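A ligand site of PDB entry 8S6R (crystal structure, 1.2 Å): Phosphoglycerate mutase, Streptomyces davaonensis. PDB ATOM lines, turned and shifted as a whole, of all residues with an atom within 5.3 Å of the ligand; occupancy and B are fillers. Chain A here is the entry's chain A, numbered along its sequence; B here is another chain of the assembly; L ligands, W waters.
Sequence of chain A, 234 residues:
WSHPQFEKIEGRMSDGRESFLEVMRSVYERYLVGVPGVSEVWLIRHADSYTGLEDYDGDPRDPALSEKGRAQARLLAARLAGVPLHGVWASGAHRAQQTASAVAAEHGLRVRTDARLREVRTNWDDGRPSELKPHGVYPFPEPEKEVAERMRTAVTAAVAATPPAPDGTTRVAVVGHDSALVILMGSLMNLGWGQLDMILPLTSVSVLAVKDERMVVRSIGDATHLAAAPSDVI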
ATOM      1  N   ARG A  45      13.241  11.394  -0.050  1.00  0.00           N
ATOM      2  CA  ARG A  45      14.365  10.575   0.405  1.00  0.00           C
ATOM      3  C   ARG A  45      15.122  11.345   1.490  1.00  0.00           C
ATOM      4  O   ARG A  45      15.337  12.560   1.381  1.00  0.00           O
ATOM      5  CB  ARG A  45      15.315  10.252  -0.720  1.00  0.00           C
ATOM      6  CG  ARG A  45      16.477   9.366  -0.252  1.00  0.00           C
ATOM      7  CD  ARG A  45      17.418   8.968  -1.351  1.00  0.00           C
ATOM      8  NE  ARG A  45      18.506   8.152  -0.803  1.00  0.00           N
ATOM      9  CZ  ARG A  45      19.675   7.943  -1.383  1.00  0.00           C
ATOM     10  NH1 ARG A  45      19.969   8.463  -2.563  1.00  0.00           N
ATOM     11  NH2 ARG A  45      20.593   7.186  -0.753  1.00  0.00           N
ATOM     12  N   HIS A  46      15.528  10.656   2.543  1.00  0.00           N
ATOM     13  CA  HIS A  46      16.294  11.329   3.592  1.00  0.00           C
ATOM     14  C   HIS A  46      17.560  11.981   3.025  1.00  0.00           C
ATOM     15  O   HIS A  46      18.029  11.701   1.918  1.00  0.00           O
ATOM     16  CB  HIS A  46      16.668  10.331   4.676  1.00  0.00           C
ATOM     17  CG  HIS A  46      17.559   9.233   4.183  1.00  0.00           C
ATOM     18  ND1 HIS A  46      18.919   9.373   4.009  1.00  0.00           N
ATOM     19  CD2 HIS A  46      17.257   7.963   3.818  1.00  0.00           C
ATOM     20  CE1 HIS A  46      19.408   8.241   3.512  1.00  0.00           C
ATOM     21  NE2 HIS A  46      18.422   7.360   3.404  1.00  0.00           N
ATOM     22  N   TYR A  50      26.039   9.245   4.613  1.00  0.00           N
ATOM     23  CA  TYR A  50      27.094   8.369   4.157  1.00  0.00           C
ATOM     24  C   TYR A  50      28.454   9.046   4.144  1.00  0.00           C
ATOM     25  O   TYR A  50      29.478   8.345   4.204  1.00  0.00           O
ATOM     26  CB  TYR A  50      26.754   7.913   2.744  1.00  0.00           C
ATOM     27  CG  TYR A  50      25.302   7.440   2.605  1.00  0.00           C
ATOM     28  CD1 TYR A  50      24.253   8.349   2.369  1.00  0.00           C
ATOM     29  CD2 TYR A  50      24.987   6.086   2.727  1.00  0.00           C
ATOM     30  CE1 TYR A  50      22.941   7.907   2.252  1.00  0.00           C
ATOM     31  CE2 TYR A  50      23.670   5.638   2.594  1.00  0.00           C
ATOM     32  CZ  TYR A  50      22.648   6.548   2.349  1.00  0.00           C
ATOM     33  OH  TYR A  50      21.354   6.072   2.213  1.00  0.00           O
ATOM     34  N   GLU A 119      13.893   1.093   4.636  1.00  0.00           N
ATOM     35  CA  GLU A 119      14.527   0.708   3.402  1.00  0.00           C
ATOM     36  C   GLU A 119      14.367  -0.792   3.178  1.00  0.00           C
ATOM     37  O   GLU A 119      14.162  -1.566   4.112  1.00  0.00           O
ATOM     38  CB  GLU A 119      16.005   1.137   3.409  1.00  0.00           C
ATOM     39  CG  GLU A 119      16.837   0.895   2.103  1.00  0.00           C
ATOM     40  CD  GLU A 119      16.245   1.488   0.829  1.00  0.00           C
ATOM     41  OE1 GLU A 119      15.085   1.195   0.479  1.00  0.00           O
ATOM     42  OE2 GLU A 119      16.967   2.244   0.102  1.00  0.00           O
ATOM     43  N   SER A 130      28.085  -6.709   0.139  1.00  0.00           N
ATOM     44  CA  SER A 130      27.264  -6.066  -0.870  1.00  0.00           C
ATOM     45  C   SER A 130      27.824  -6.386  -2.248  1.00  0.00           C
ATOM     46  O   SER A 130      29.018  -6.590  -2.418  1.00  0.00           O
ATOM     47  CB  SER A 130      27.309  -4.550  -0.654  1.00  0.00           C
ATOM     48  OG  SER A 130      26.728  -4.202   0.597  1.00  0.00           O
ATOM     49  N   GLU A 131      26.928  -6.430  -3.240  1.00  0.00           N
ATOM     50  CA  GLU A 131      27.358  -6.722  -4.601  1.00  0.00           C
ATOM     51  C   GLU A 131      26.714  -5.717  -5.553  1.00  0.00           C
ATOM     52  O   GLU A 131      25.519  -5.432  -5.439  1.00  0.00           O
ATOM     53  CB  GLU A 131      26.876  -8.117  -5.056  1.00  0.00           C
ATOM     54  CG  GLU A 131      27.374  -9.268  -4.208  1.00  0.00           C
ATOM     55  CD  GLU A 131      26.813 -10.597  -4.663  1.00  0.00           C
ATOM     56  OE1 GLU A 131      26.349 -10.663  -5.821  1.00  0.00           O
ATOM     57  OE2 GLU A 131      26.827 -11.555  -3.868  1.00  0.00           O
ATOM     58  N   LEU A 132      27.494  -5.229  -6.511  1.00  0.00           N
ATOM     59  CA  LEU A 132      26.947  -4.432  -7.613  1.00  0.00           C
ATOM     60  C   LEU A 132      26.331  -5.357  -8.657  1.00  0.00           C
ATOM     61  O   LEU A 132      27.018  -6.211  -9.232  1.00  0.00           O
ATOM     62  CB  LEU A 132      28.067  -3.586  -8.228  1.00  0.00           C
ATOM     63  CG  LEU A 132      27.650  -2.798  -9.477  1.00  0.00           C
ATOM     64  CD1 LEU A 132      26.638  -1.758  -9.110  1.00  0.00           C
ATOM     65  CD2 LEU A 132      28.853  -2.138 -10.078  1.00  0.00           C
ATOM     66  N   LYS A 133      25.014  -5.208  -8.910  1.00  0.00           N
ATOM     67  CA  LYS A 133      24.322  -6.086  -9.839  1.00  0.00           C
ATOM     68  C   LYS A 133      24.169  -5.387 -11.187  1.00  0.00           C
ATOM     69  O   LYS A 133      24.091  -4.159 -11.254  1.00  0.00           O
ATOM     70  CB  LYS A 133      22.931  -6.409  -9.321  1.00  0.00           C
ATOM     71  CG  LYS A 133      22.894  -7.407  -8.147  1.00  0.00           C
ATOM     72  CD  LYS A 133      23.797  -8.598  -8.466  1.00  0.00           C
ATOM     73  CE  LYS A 133      23.366  -9.863  -7.782  1.00  0.00           C
ATOM     74  NZ  LYS A 133      24.227 -10.986  -8.282  1.00  0.00           N
ATOM     75  N   PRO A 139      18.725  -6.629  -6.569  1.00  0.00           N
ATOM     76  CA  PRO A 139      19.931  -6.781  -5.733  1.00  0.00           C
ATOM     77  C   PRO A 139      19.654  -7.002  -4.248  1.00  0.00           C
ATOM     78  O   PRO A 139      20.621  -7.039  -3.459  1.00  0.00           O
ATOM     79  CB  PRO A 139      20.621  -5.435  -5.937  1.00  0.00           C
ATOM     80  CG  PRO A 139      19.491  -4.479  -6.094  1.00  0.00           C
ATOM     81  CD  PRO A 139      18.415  -5.217  -6.854  1.00  0.00           C
ATOM     82  N   PHE A 140      18.402  -7.166  -3.822  1.00  0.00           N
ATOM     83  CA  PHE A 140      18.123  -7.172  -2.399  1.00  0.00           C
ATOM     84  C   PHE A 140      17.540  -8.497  -1.935  1.00  0.00           C
ATOM     85  O   PHE A 140      16.841  -9.185  -2.696  1.00  0.00           O
ATOM     86  CB  PHE A 140      17.115  -6.068  -2.052  1.00  0.00           C
ATOM     87  CG  PHE A 140      17.485  -4.743  -2.618  1.00  0.00           C
ATOM     88  CD1 PHE A 140      18.611  -4.065  -2.167  1.00  0.00           C
ATOM     89  CD2 PHE A 140      16.699  -4.168  -3.599  1.00  0.00           C
ATOM     90  CE1 PHE A 140      18.975  -2.833  -2.721  1.00  0.00           C
ATOM     91  CE2 PHE A 140      17.030  -2.909  -4.160  1.00  0.00           C
ATOM     92  CZ  PHE A 140      18.183  -2.235  -3.696  1.00  0.00           C
ATOM     93  N   HIS A 177      13.339   5.987   1.957  1.00  0.00           N
ATOM     94  CA  HIS A 177      14.639   5.536   1.501  1.00  0.00           C
ATOM     95  C   HIS A 177      14.565   5.222   0.015  1.00  0.00           C
ATOM     96  O   HIS A 177      13.538   4.740  -0.485  1.00  0.00           O
ATOM     97  CB  HIS A 177      15.054   4.288   2.308  1.00  0.00           C
ATOM     98  CG  HIS A 177      15.119   4.566   3.784  1.00  0.00           C
ATOM     99  ND1 HIS A 177      16.295   4.882   4.456  1.00  0.00           N
ATOM    100  CD2 HIS A 177      14.152   4.553   4.734  1.00  0.00           C
ATOM    101  CE1 HIS A 177      16.035   5.086   5.728  1.00  0.00           C
ATOM    102  NE2 HIS A 177      14.734   4.897   5.935  1.00  0.00           N
ATOM    103  N   ASP A 178      15.670   5.478  -0.678  1.00  0.00           N
ATOM    104  CA  ASP A 178      15.715   5.379  -2.129  1.00  0.00           C
ATOM    105  C   ASP A 178      15.031   4.130  -2.673  1.00  0.00           C
ATOM    106  O   ASP A 178      14.098   4.245  -3.483  1.00  0.00           O
ATOM    107  CB  ASP A 178      17.183   5.405  -2.557  1.00  0.00           C
ATOM    108  CG  ASP A 178      17.376   4.956  -3.984  1.00  0.00           C
ATOM    109  OD1 ASP A 178      16.728   5.590  -4.856  1.00  0.00           O
ATOM    110  OD2 ASP A 178      18.154   4.006  -4.209  1.00  0.00           O
ATOM    111  N   SER A 179      15.556   2.949  -2.376  1.00  0.00           N
ATOM    112  CA  SER A 179      15.124   1.790  -3.156  1.00  0.00           C
ATOM    113  C   SER A 179      13.671   1.424  -2.853  1.00  0.00           C
ATOM    114  O   SER A 179      12.920   1.070  -3.778  1.00  0.00           O
ATOM    115  CB  SER A 179      16.072   0.615  -2.910  1.00  0.00           C
ATOM    116  OG  SER A 179      17.367   0.991  -3.418  1.00  0.00           O
ATOM    117  N   VAL A 182      11.572   3.846  -4.837  1.00  0.00           N
ATOM    118  CA  VAL A 182      11.586   3.491  -6.270  1.00  0.00           C
ATOM    119  C   VAL A 182      10.726   2.253  -6.532  1.00  0.00           C
ATOM    120  O   VAL A 182      10.029   2.168  -7.564  1.00  0.00           O
ATOM    121  CB  VAL A 182      13.040   3.297  -6.776  1.00  0.00           C
ATOM    122  CG1 VAL A 182      13.060   2.664  -8.169  1.00  0.00           C
ATOM    123  CG2 VAL A 182      13.796   4.640  -6.786  1.00  0.00           C
ATOM    124  N   TRP A 193      11.472  -3.937 -10.917  1.00  0.00           N
ATOM    125  CA  TRP A 193      12.738  -3.279 -10.610  1.00  0.00           C
ATOM    126  C   TRP A 193      13.595  -3.241 -11.864  1.00  0.00           C
ATOM    127  O   TRP A 193      13.782  -4.239 -12.550  1.00  0.00           O
ATOM    128  CB  TRP A 193      13.463  -4.094  -9.538  1.00  0.00           C
ATOM    129  CG  TRP A 193      14.841  -3.494  -9.173  1.00  0.00           C
ATOM    130  CD1 TRP A 193      16.042  -3.893  -9.670  1.00  0.00           C
ATOM    131  CD2 TRP A 193      15.110  -2.414  -8.248  1.00  0.00           C
ATOM    132  NE1 TRP A 193      17.049  -3.105  -9.133  1.00  0.00           N
ATOM    133  CE2 TRP A 193      16.509  -2.209  -8.246  1.00  0.00           C
ATOM    134  CE3 TRP A 193      14.318  -1.596  -7.414  1.00  0.00           C
ATOM    135  CZ2 TRP A 193      17.134  -1.237  -7.481  1.00  0.00           C
ATOM    136  CZ3 TRP A 193      14.941  -0.588  -6.649  1.00  0.00           C
ATOM    137  CH2 TRP A 193      16.362  -0.428  -6.701  1.00  0.00           C
ATOM    138  N   ASP A 197      14.242   3.237 -14.024  1.00  0.00           N
ATOM    139  CA  ASP A 197      15.670   3.014 -13.765  1.00  0.00           C
ATOM    140  C   ASP A 197      16.288   4.295 -13.212  1.00  0.00           C
ATOM    141  O   ASP A 197      16.873   5.066 -13.967  1.00  0.00           O
ATOM    142  CB  ASP A 197      16.350   2.626 -15.083  1.00  0.00           C
ATOM    143  CG  ASP A 197      17.805   2.278 -14.900  1.00  0.00           C
ATOM    144  OD1 ASP A 197      18.131   1.844 -13.772  1.00  0.00           O
ATOM    145  OD2 ASP A 197      18.573   2.442 -15.858  1.00  0.00           O
ATOM    146  N   MET A 198      16.104   4.526 -11.910  1.00  0.00           N
ATOM    147  CA  MET A 198      16.464   5.803 -11.302  1.00  0.00           C
ATOM    148  C   MET A 198      16.971   5.568  -9.889  1.00  0.00           C
ATOM    149  O   MET A 198      16.496   4.659  -9.186  1.00  0.00           O
ATOM    150  CB  MET A 198      15.202   6.675 -11.199  1.00  0.00           C
ATOM    151  CG  MET A 198      14.680   7.116 -12.533  1.00  0.00           C
ATOM    152  SD  MET A 198      13.101   8.057 -12.494  1.00  0.00           S
ATOM    153  CE  MET A 198      13.760   9.641 -11.992  1.00  0.00           C
ATOM    154  N   ILE A 199      17.946   6.378  -9.466  1.00  0.00           N
ATOM    155  CA  ILE A 199      18.288   6.510  -8.058  1.00  0.00           C
ATOM    156  C   ILE A 199      17.768   7.866  -7.593  1.00  0.00           C
ATOM    157  O   ILE A 199      18.072   8.899  -8.206  1.00  0.00           O
ATOM    158  CB  ILE A 199      19.786   6.326  -7.784  1.00  0.00           C
ATOM    159  CG1 ILE A 199      20.089   6.513  -6.282  1.00  0.00           C
ATOM    160  CG2 ILE A 199      20.613   7.226  -8.573  1.00  0.00           C
ATOM    161  CD1 ILE A 199      21.331   5.724  -5.824  1.00  0.00           C
ATOM    162  N   LEU A 200      16.983   7.880  -6.562  1.00  0.00           N
ATOM    163  CA  LEU A 200      16.387   9.123  -6.100  1.00  0.00           C
ATOM    164  C   LEU A 200      17.448   9.952  -5.370  1.00  0.00           C
ATOM    165  O   LEU A 200      18.134   9.436  -4.452  1.00  0.00           O
ATOM    166  CB  LEU A 200      15.220   8.862  -5.167  1.00  0.00           C
ATOM    167  CG  LEU A 200      14.105   8.051  -5.784  1.00  0.00           C
ATOM    168  CD1 LEU A 200      13.058   7.773  -4.740  1.00  0.00           C
ATOM    169  CD2 LEU A 200      13.464   8.780  -6.979  1.00  0.00           C
ATOM    170  N   PHE B  20      29.541  -2.102   1.382  1.00  0.00           N
ATOM    171  CA  PHE B  20      28.337  -1.328   1.105  1.00  0.00           C
ATOM    172  C   PHE B  20      28.657  -0.006   0.414  1.00  0.00           C
ATOM    173  O   PHE B  20      28.021   0.358  -0.584  1.00  0.00           O
ATOM    174  CB  PHE B  20      27.569  -1.101   2.403  1.00  0.00           C
ATOM    175  CG  PHE B  20      26.302  -0.268   2.194  1.00  0.00           C
ATOM    176  CD1 PHE B  20      25.137  -0.891   1.772  1.00  0.00           C
ATOM    177  CD2 PHE B  20      26.299   1.095   2.419  1.00  0.00           C
ATOM    178  CE1 PHE B  20      23.967  -0.169   1.588  1.00  0.00           C
ATOM    179  CE2 PHE B  20      25.144   1.836   2.217  1.00  0.00           C
ATOM    180  CZ  PHE B  20      23.974   1.201   1.800  1.00  0.00           C
ATOM    181  N   VAL B  23      29.927  -0.365  -3.230  1.00  0.00           N
ATOM    182  CA  VAL B  23      28.826  -0.623  -4.160  1.00  0.00           C
ATOM    183  C   VAL B  23      27.962   0.625  -4.345  1.00  0.00           C
ATOM    184  O   VAL B  23      27.605   0.987  -5.487  1.00  0.00           O
ATOM    185  CB  VAL B  23      28.013  -1.845  -3.676  1.00  0.00           C
ATOM    186  CG1 VAL B  23      26.747  -1.997  -4.544  1.00  0.00           C
ATOM    187  CG2 VAL B  23      28.820  -3.049  -3.813  1.00  0.00           C
ATOM    188  N   MET B  24      27.652   1.324  -3.248  1.00  0.00           N
ATOM    189  CA  MET B  24      26.844   2.540  -3.335  1.00  0.00           C
ATOM    190  C   MET B  24      27.496   3.553  -4.275  1.00  0.00           C
ATOM    191  O   MET B  24      26.806   4.202  -5.069  1.00  0.00           O
ATOM    192  CB  MET B  24      26.670   3.159  -1.960  1.00  0.00           C
ATOM    193  CG  MET B  24      25.743   4.368  -1.956  1.00  0.00           C
ATOM    194  SD  MET B  24      25.655   5.181  -0.379  1.00  0.00           S
ATOM    195  CE  MET B  24      27.287   5.890  -0.264  1.00  0.00           C
ATOM    196  N   VAL B  27      27.072   2.400  -7.918  1.00  0.00           N
ATOM    197  CA  VAL B  27      25.718   2.657  -8.401  1.00  0.00           C
ATOM    198  C   VAL B  27      25.549   4.130  -8.720  1.00  0.00           C
ATOM    199  O   VAL B  27      25.109   4.488  -9.822  1.00  0.00           O
ATOM    200  CB  VAL B  27      24.693   2.172  -7.348  1.00  0.00           C
ATOM    201  CG1 VAL B  27      23.234   2.637  -7.704  1.00  0.00           C
ATOM    202  CG2 VAL B  27      24.727   0.652  -7.194  1.00  0.00           C
ATOM    203  N   TYR B  31      24.618   6.373 -12.583  1.00  0.00           N
ATOM    204  CA  TYR B  31      23.571   7.357 -12.802  1.00  0.00           C
ATOM    205  C   TYR B  31      24.101   8.779 -12.734  1.00  0.00           C
ATOM    206  O   TYR B  31      23.332   9.719 -12.572  1.00  0.00           O
ATOM    207  CB  TYR B  31      22.420   7.131 -11.836  1.00  0.00           C
ATOM    208  CG  TYR B  31      21.861   5.731 -12.032  1.00  0.00           C
ATOM    209  CD1 TYR B  31      20.911   5.504 -12.996  1.00  0.00           C
ATOM    210  CD2 TYR B  31      22.372   4.651 -11.332  1.00  0.00           C
ATOM    211  CE1 TYR B  31      20.434   4.207 -13.238  1.00  0.00           C
ATOM    212  CE2 TYR B  31      21.926   3.367 -11.525  1.00  0.00           C
ATOM    213  CZ  TYR B  31      20.941   3.150 -12.481  1.00  0.00           C
ATOM    214  OH  TYR B  31      20.478   1.859 -12.750  1.00  0.00           O
HETATM  215  O1  LIG L   1      23.400  -3.379  -7.751  1.00  0.00           O
HETATM  216  C1  LIG L   1      23.054  -2.827  -6.542  1.00  0.00           C
HETATM  217  N1  LIG L   1      23.576  -3.319  -5.440  1.00  0.00           N
HETATM  218  C2  LIG L   1      23.266  -2.771  -4.260  1.00  0.00           C
HETATM  219  O2  LIG L   1      23.754  -3.363  -3.166  1.00  0.00           O
HETATM  220  C3  LIG L   1      22.124  -1.769  -6.440  1.00  0.00           C
HETATM  221  C4  LIG L   1      21.909  -1.204  -5.218  1.00  0.00           C
HETATM  222  N2  LIG L   1      22.441  -1.776  -4.101  1.00  0.00           N
HETATM  223  N3  LIG L   1      21.660  -1.192  -7.644  1.00  0.00           N
HETATM  224  C5  LIG L   1      20.807  -0.130  -7.490  1.00  0.00           C
HETATM  225  C6  LIG L   1      20.224   0.503  -8.660  1.00  0.00           C
HETATM  226  C7  LIG L   1      19.354   1.593  -8.530  1.00  0.00           C
HETATM  227  C8  LIG L   1      18.797   2.344  -9.779  1.00  0.00           C
HETATM  228  C9  LIG L   1      18.991   2.005  -7.262  1.00  0.00           C
HETATM  229  N4  LIG L   1      18.019   3.078  -7.082  1.00  0.00           N
HETATM  230  C10 LIG L   1      19.540   1.405  -6.120  1.00  0.00           C
HETATM  231  C11 LIG L   1      20.498   0.377  -6.223  1.00  0.00           C
HETATM  232  N5  LIG L   1      21.084  -0.129  -5.065  1.00  0.00           N
HETATM  233  C12 LIG L   1      20.891   0.454  -3.774  1.00  0.00           C
HETATM  234  C13 LIG L   1      21.790   1.747  -3.654  1.00  0.00           C
HETATM  235  O3  LIG L   1      23.153   1.472  -3.979  1.00  0.00           O
HETATM  236  C14 LIG L   1      21.816   2.255  -2.190  1.00  0.00           C
HETATM  237  O4  LIG L   1      22.216   1.208  -1.281  1.00  0.00           O
HETATM  238  C15 LIG L   1      20.444   2.812  -1.797  1.00  0.00           C
HETATM  239  O5  LIG L   1      20.341   3.979  -2.599  1.00  0.00           O
HETATM  240  C16 LIG L   1      20.432   3.173  -0.270  1.00  0.00           C
HETATM  241  O6  LIG L   1      19.156   3.625   0.256  1.00  0.00           O
HETATM  242  O   HOH W   1      18.726   0.271  -0.827  1.00  0.00           O
HETATM  243  O   HOH W   2      24.838  -0.129  -1.886  1.00  0.00           O
HETATM  244  O   HOH W   3      15.912   0.796  -9.768  1.00  0.00           O
HETATM  245  O   HOH W   4      23.916   4.449  -4.516  1.00  0.00           O
HETATM  246  O   HOH W   5      24.211  -5.787  -2.436  1.00  0.00           O
HETATM  247  O   HOH W   6      22.378  -3.047  -0.902  1.00  0.00           O
HETATM  248  O   HOH W   7      22.296   5.817  -2.644  1.00  0.00           O
HETATM  249  O   HOH W   8      18.007   5.980   0.978  1.00  0.00           O
HETATM  250  O   HOH W   9      18.976   3.806   3.334  1.00  0.00           O
HETATM  251  O   HOH W  10      22.164  -2.376 -10.167  1.00  0.00           O
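An oxygen (O6) of the ligand is in hydrogen-bond range of the side-chain carboxylate (OE2) of Glu 119 (2.6 Å). An oxygen (O1) of the ligand is in hydrogen-bond range of the backbone NH (N) of Lys 133 (2.7 Å). The side-chain carboxylate of Asp 178 is in hydrogen-bond range of an oxygen (O5) of the ligand (2.7 Å). The backbone carbonyl oxygen (O) of Glu 131 sits at hydrogen-bond distance from a nitrogen (N1) of the ligand, 2.9 Å away.
The side-chain carboxylate (OE2) of Glu 119 is in hydrogen-bond range of the backbone NH (N) of Ser 179, 2.9 Å away. NZ of Lys 133 lies within salt-bridge range of OE1 of Glu 131. The side-chain carboxylate (OD2) of Asp 178 is in hydrogen-bond range of the side-chain hydroxyl (OG) of Ser 179, 3.2 Å away. OD1 of Asp 178 is in hydrogen-bond range of N of Leu 200, 2.9 Å away. The side-chain hydroxyl (OH) of Tyr 31 of chain B sits at hydrogen-bond distance from the side-chain carboxylate (OD1) of Asp 197 (2.6 Å). The side-chain hydroxyl (OH) of Tyr 50 lies within hydrogen-bond range of the guanidinium group (NH2) of Arg 45. NH1 of Arg 45 sits at hydrogen-bond distance from O of Leu 200 (2.8 Å). A ring nitrogen (NE2) of His 46 sits close to the side-chain hydroxyl of Tyr 50.
The backbone carbonyl oxygen (O) of Met 198 sits close to a nitrogen (N4) of the ligand, at 3.0 Å. Arg 45 touches the ligand. Tyr 50 touches the ligand. Leu 132 touches the ligand (C to O1, 3.7 Å). Pro 139 touches the ligand (CB to C1, 3.6 Å). CZ of Phe 140 touches C12 of the ligand, 3.8 Å away. Ser 179 touches the ligand (OG to C10, 3.5 Å). Trp 193 touches the ligand. Ile 199 touches the ligand (CA to N4, 3.6 Å). Phe 20 of chain B touches the ligand. Val 23 of chain B touches the ligand. Met 24 of chain B touches the ligand. Val 27 of chain B touches the ligand. Tyr 31 of chain B touches the ligand (OH to C8, 3.4 Å). Hydrophobic or aromatic side chains within 4 Å of the ligand: Leu 132, Pro 139, Phe 140, Trp 193, Ile 199, Phe 20 of chain B, Val 23 of chain B, Val 27 of chain B and Tyr 31 of chain B. Of the 24 residues printed, 18 come within 4 Å of the ligand.
Water W5 lies within hydrogen-bond range of an oxygen (O2) of the ligand (2.6 Å) and the backbone NH of Glu 131 (2.9 Å). Water W7 bridges an oxygen (O5) of the ligand (2.7 Å) and the guanidinium group (NH2) of Arg 45 (2.9 Å). Water W10 bridges N3 of the ligand (2.8 Å) and O of Lys 133 (2.8 Å). Water W2 lies within hydrogen-bond range of an oxygen (O4) of the ligand, the backbone NH (N) of Met 24 of chain B and the backbone carbonyl oxygen (O) of Phe 20 of chain B. Water W4 lies within hydrogen-bond range of the backbone carbonyl oxygen (O) of Met 24 of chain B and an oxygen (O3) of the ligand. Water W1 bridges the side-chain carboxylate (OE2) of Glu 119 (2.8 Å) and the side-chain hydroxyl (OG) of Ser 179 (3.0 Å).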
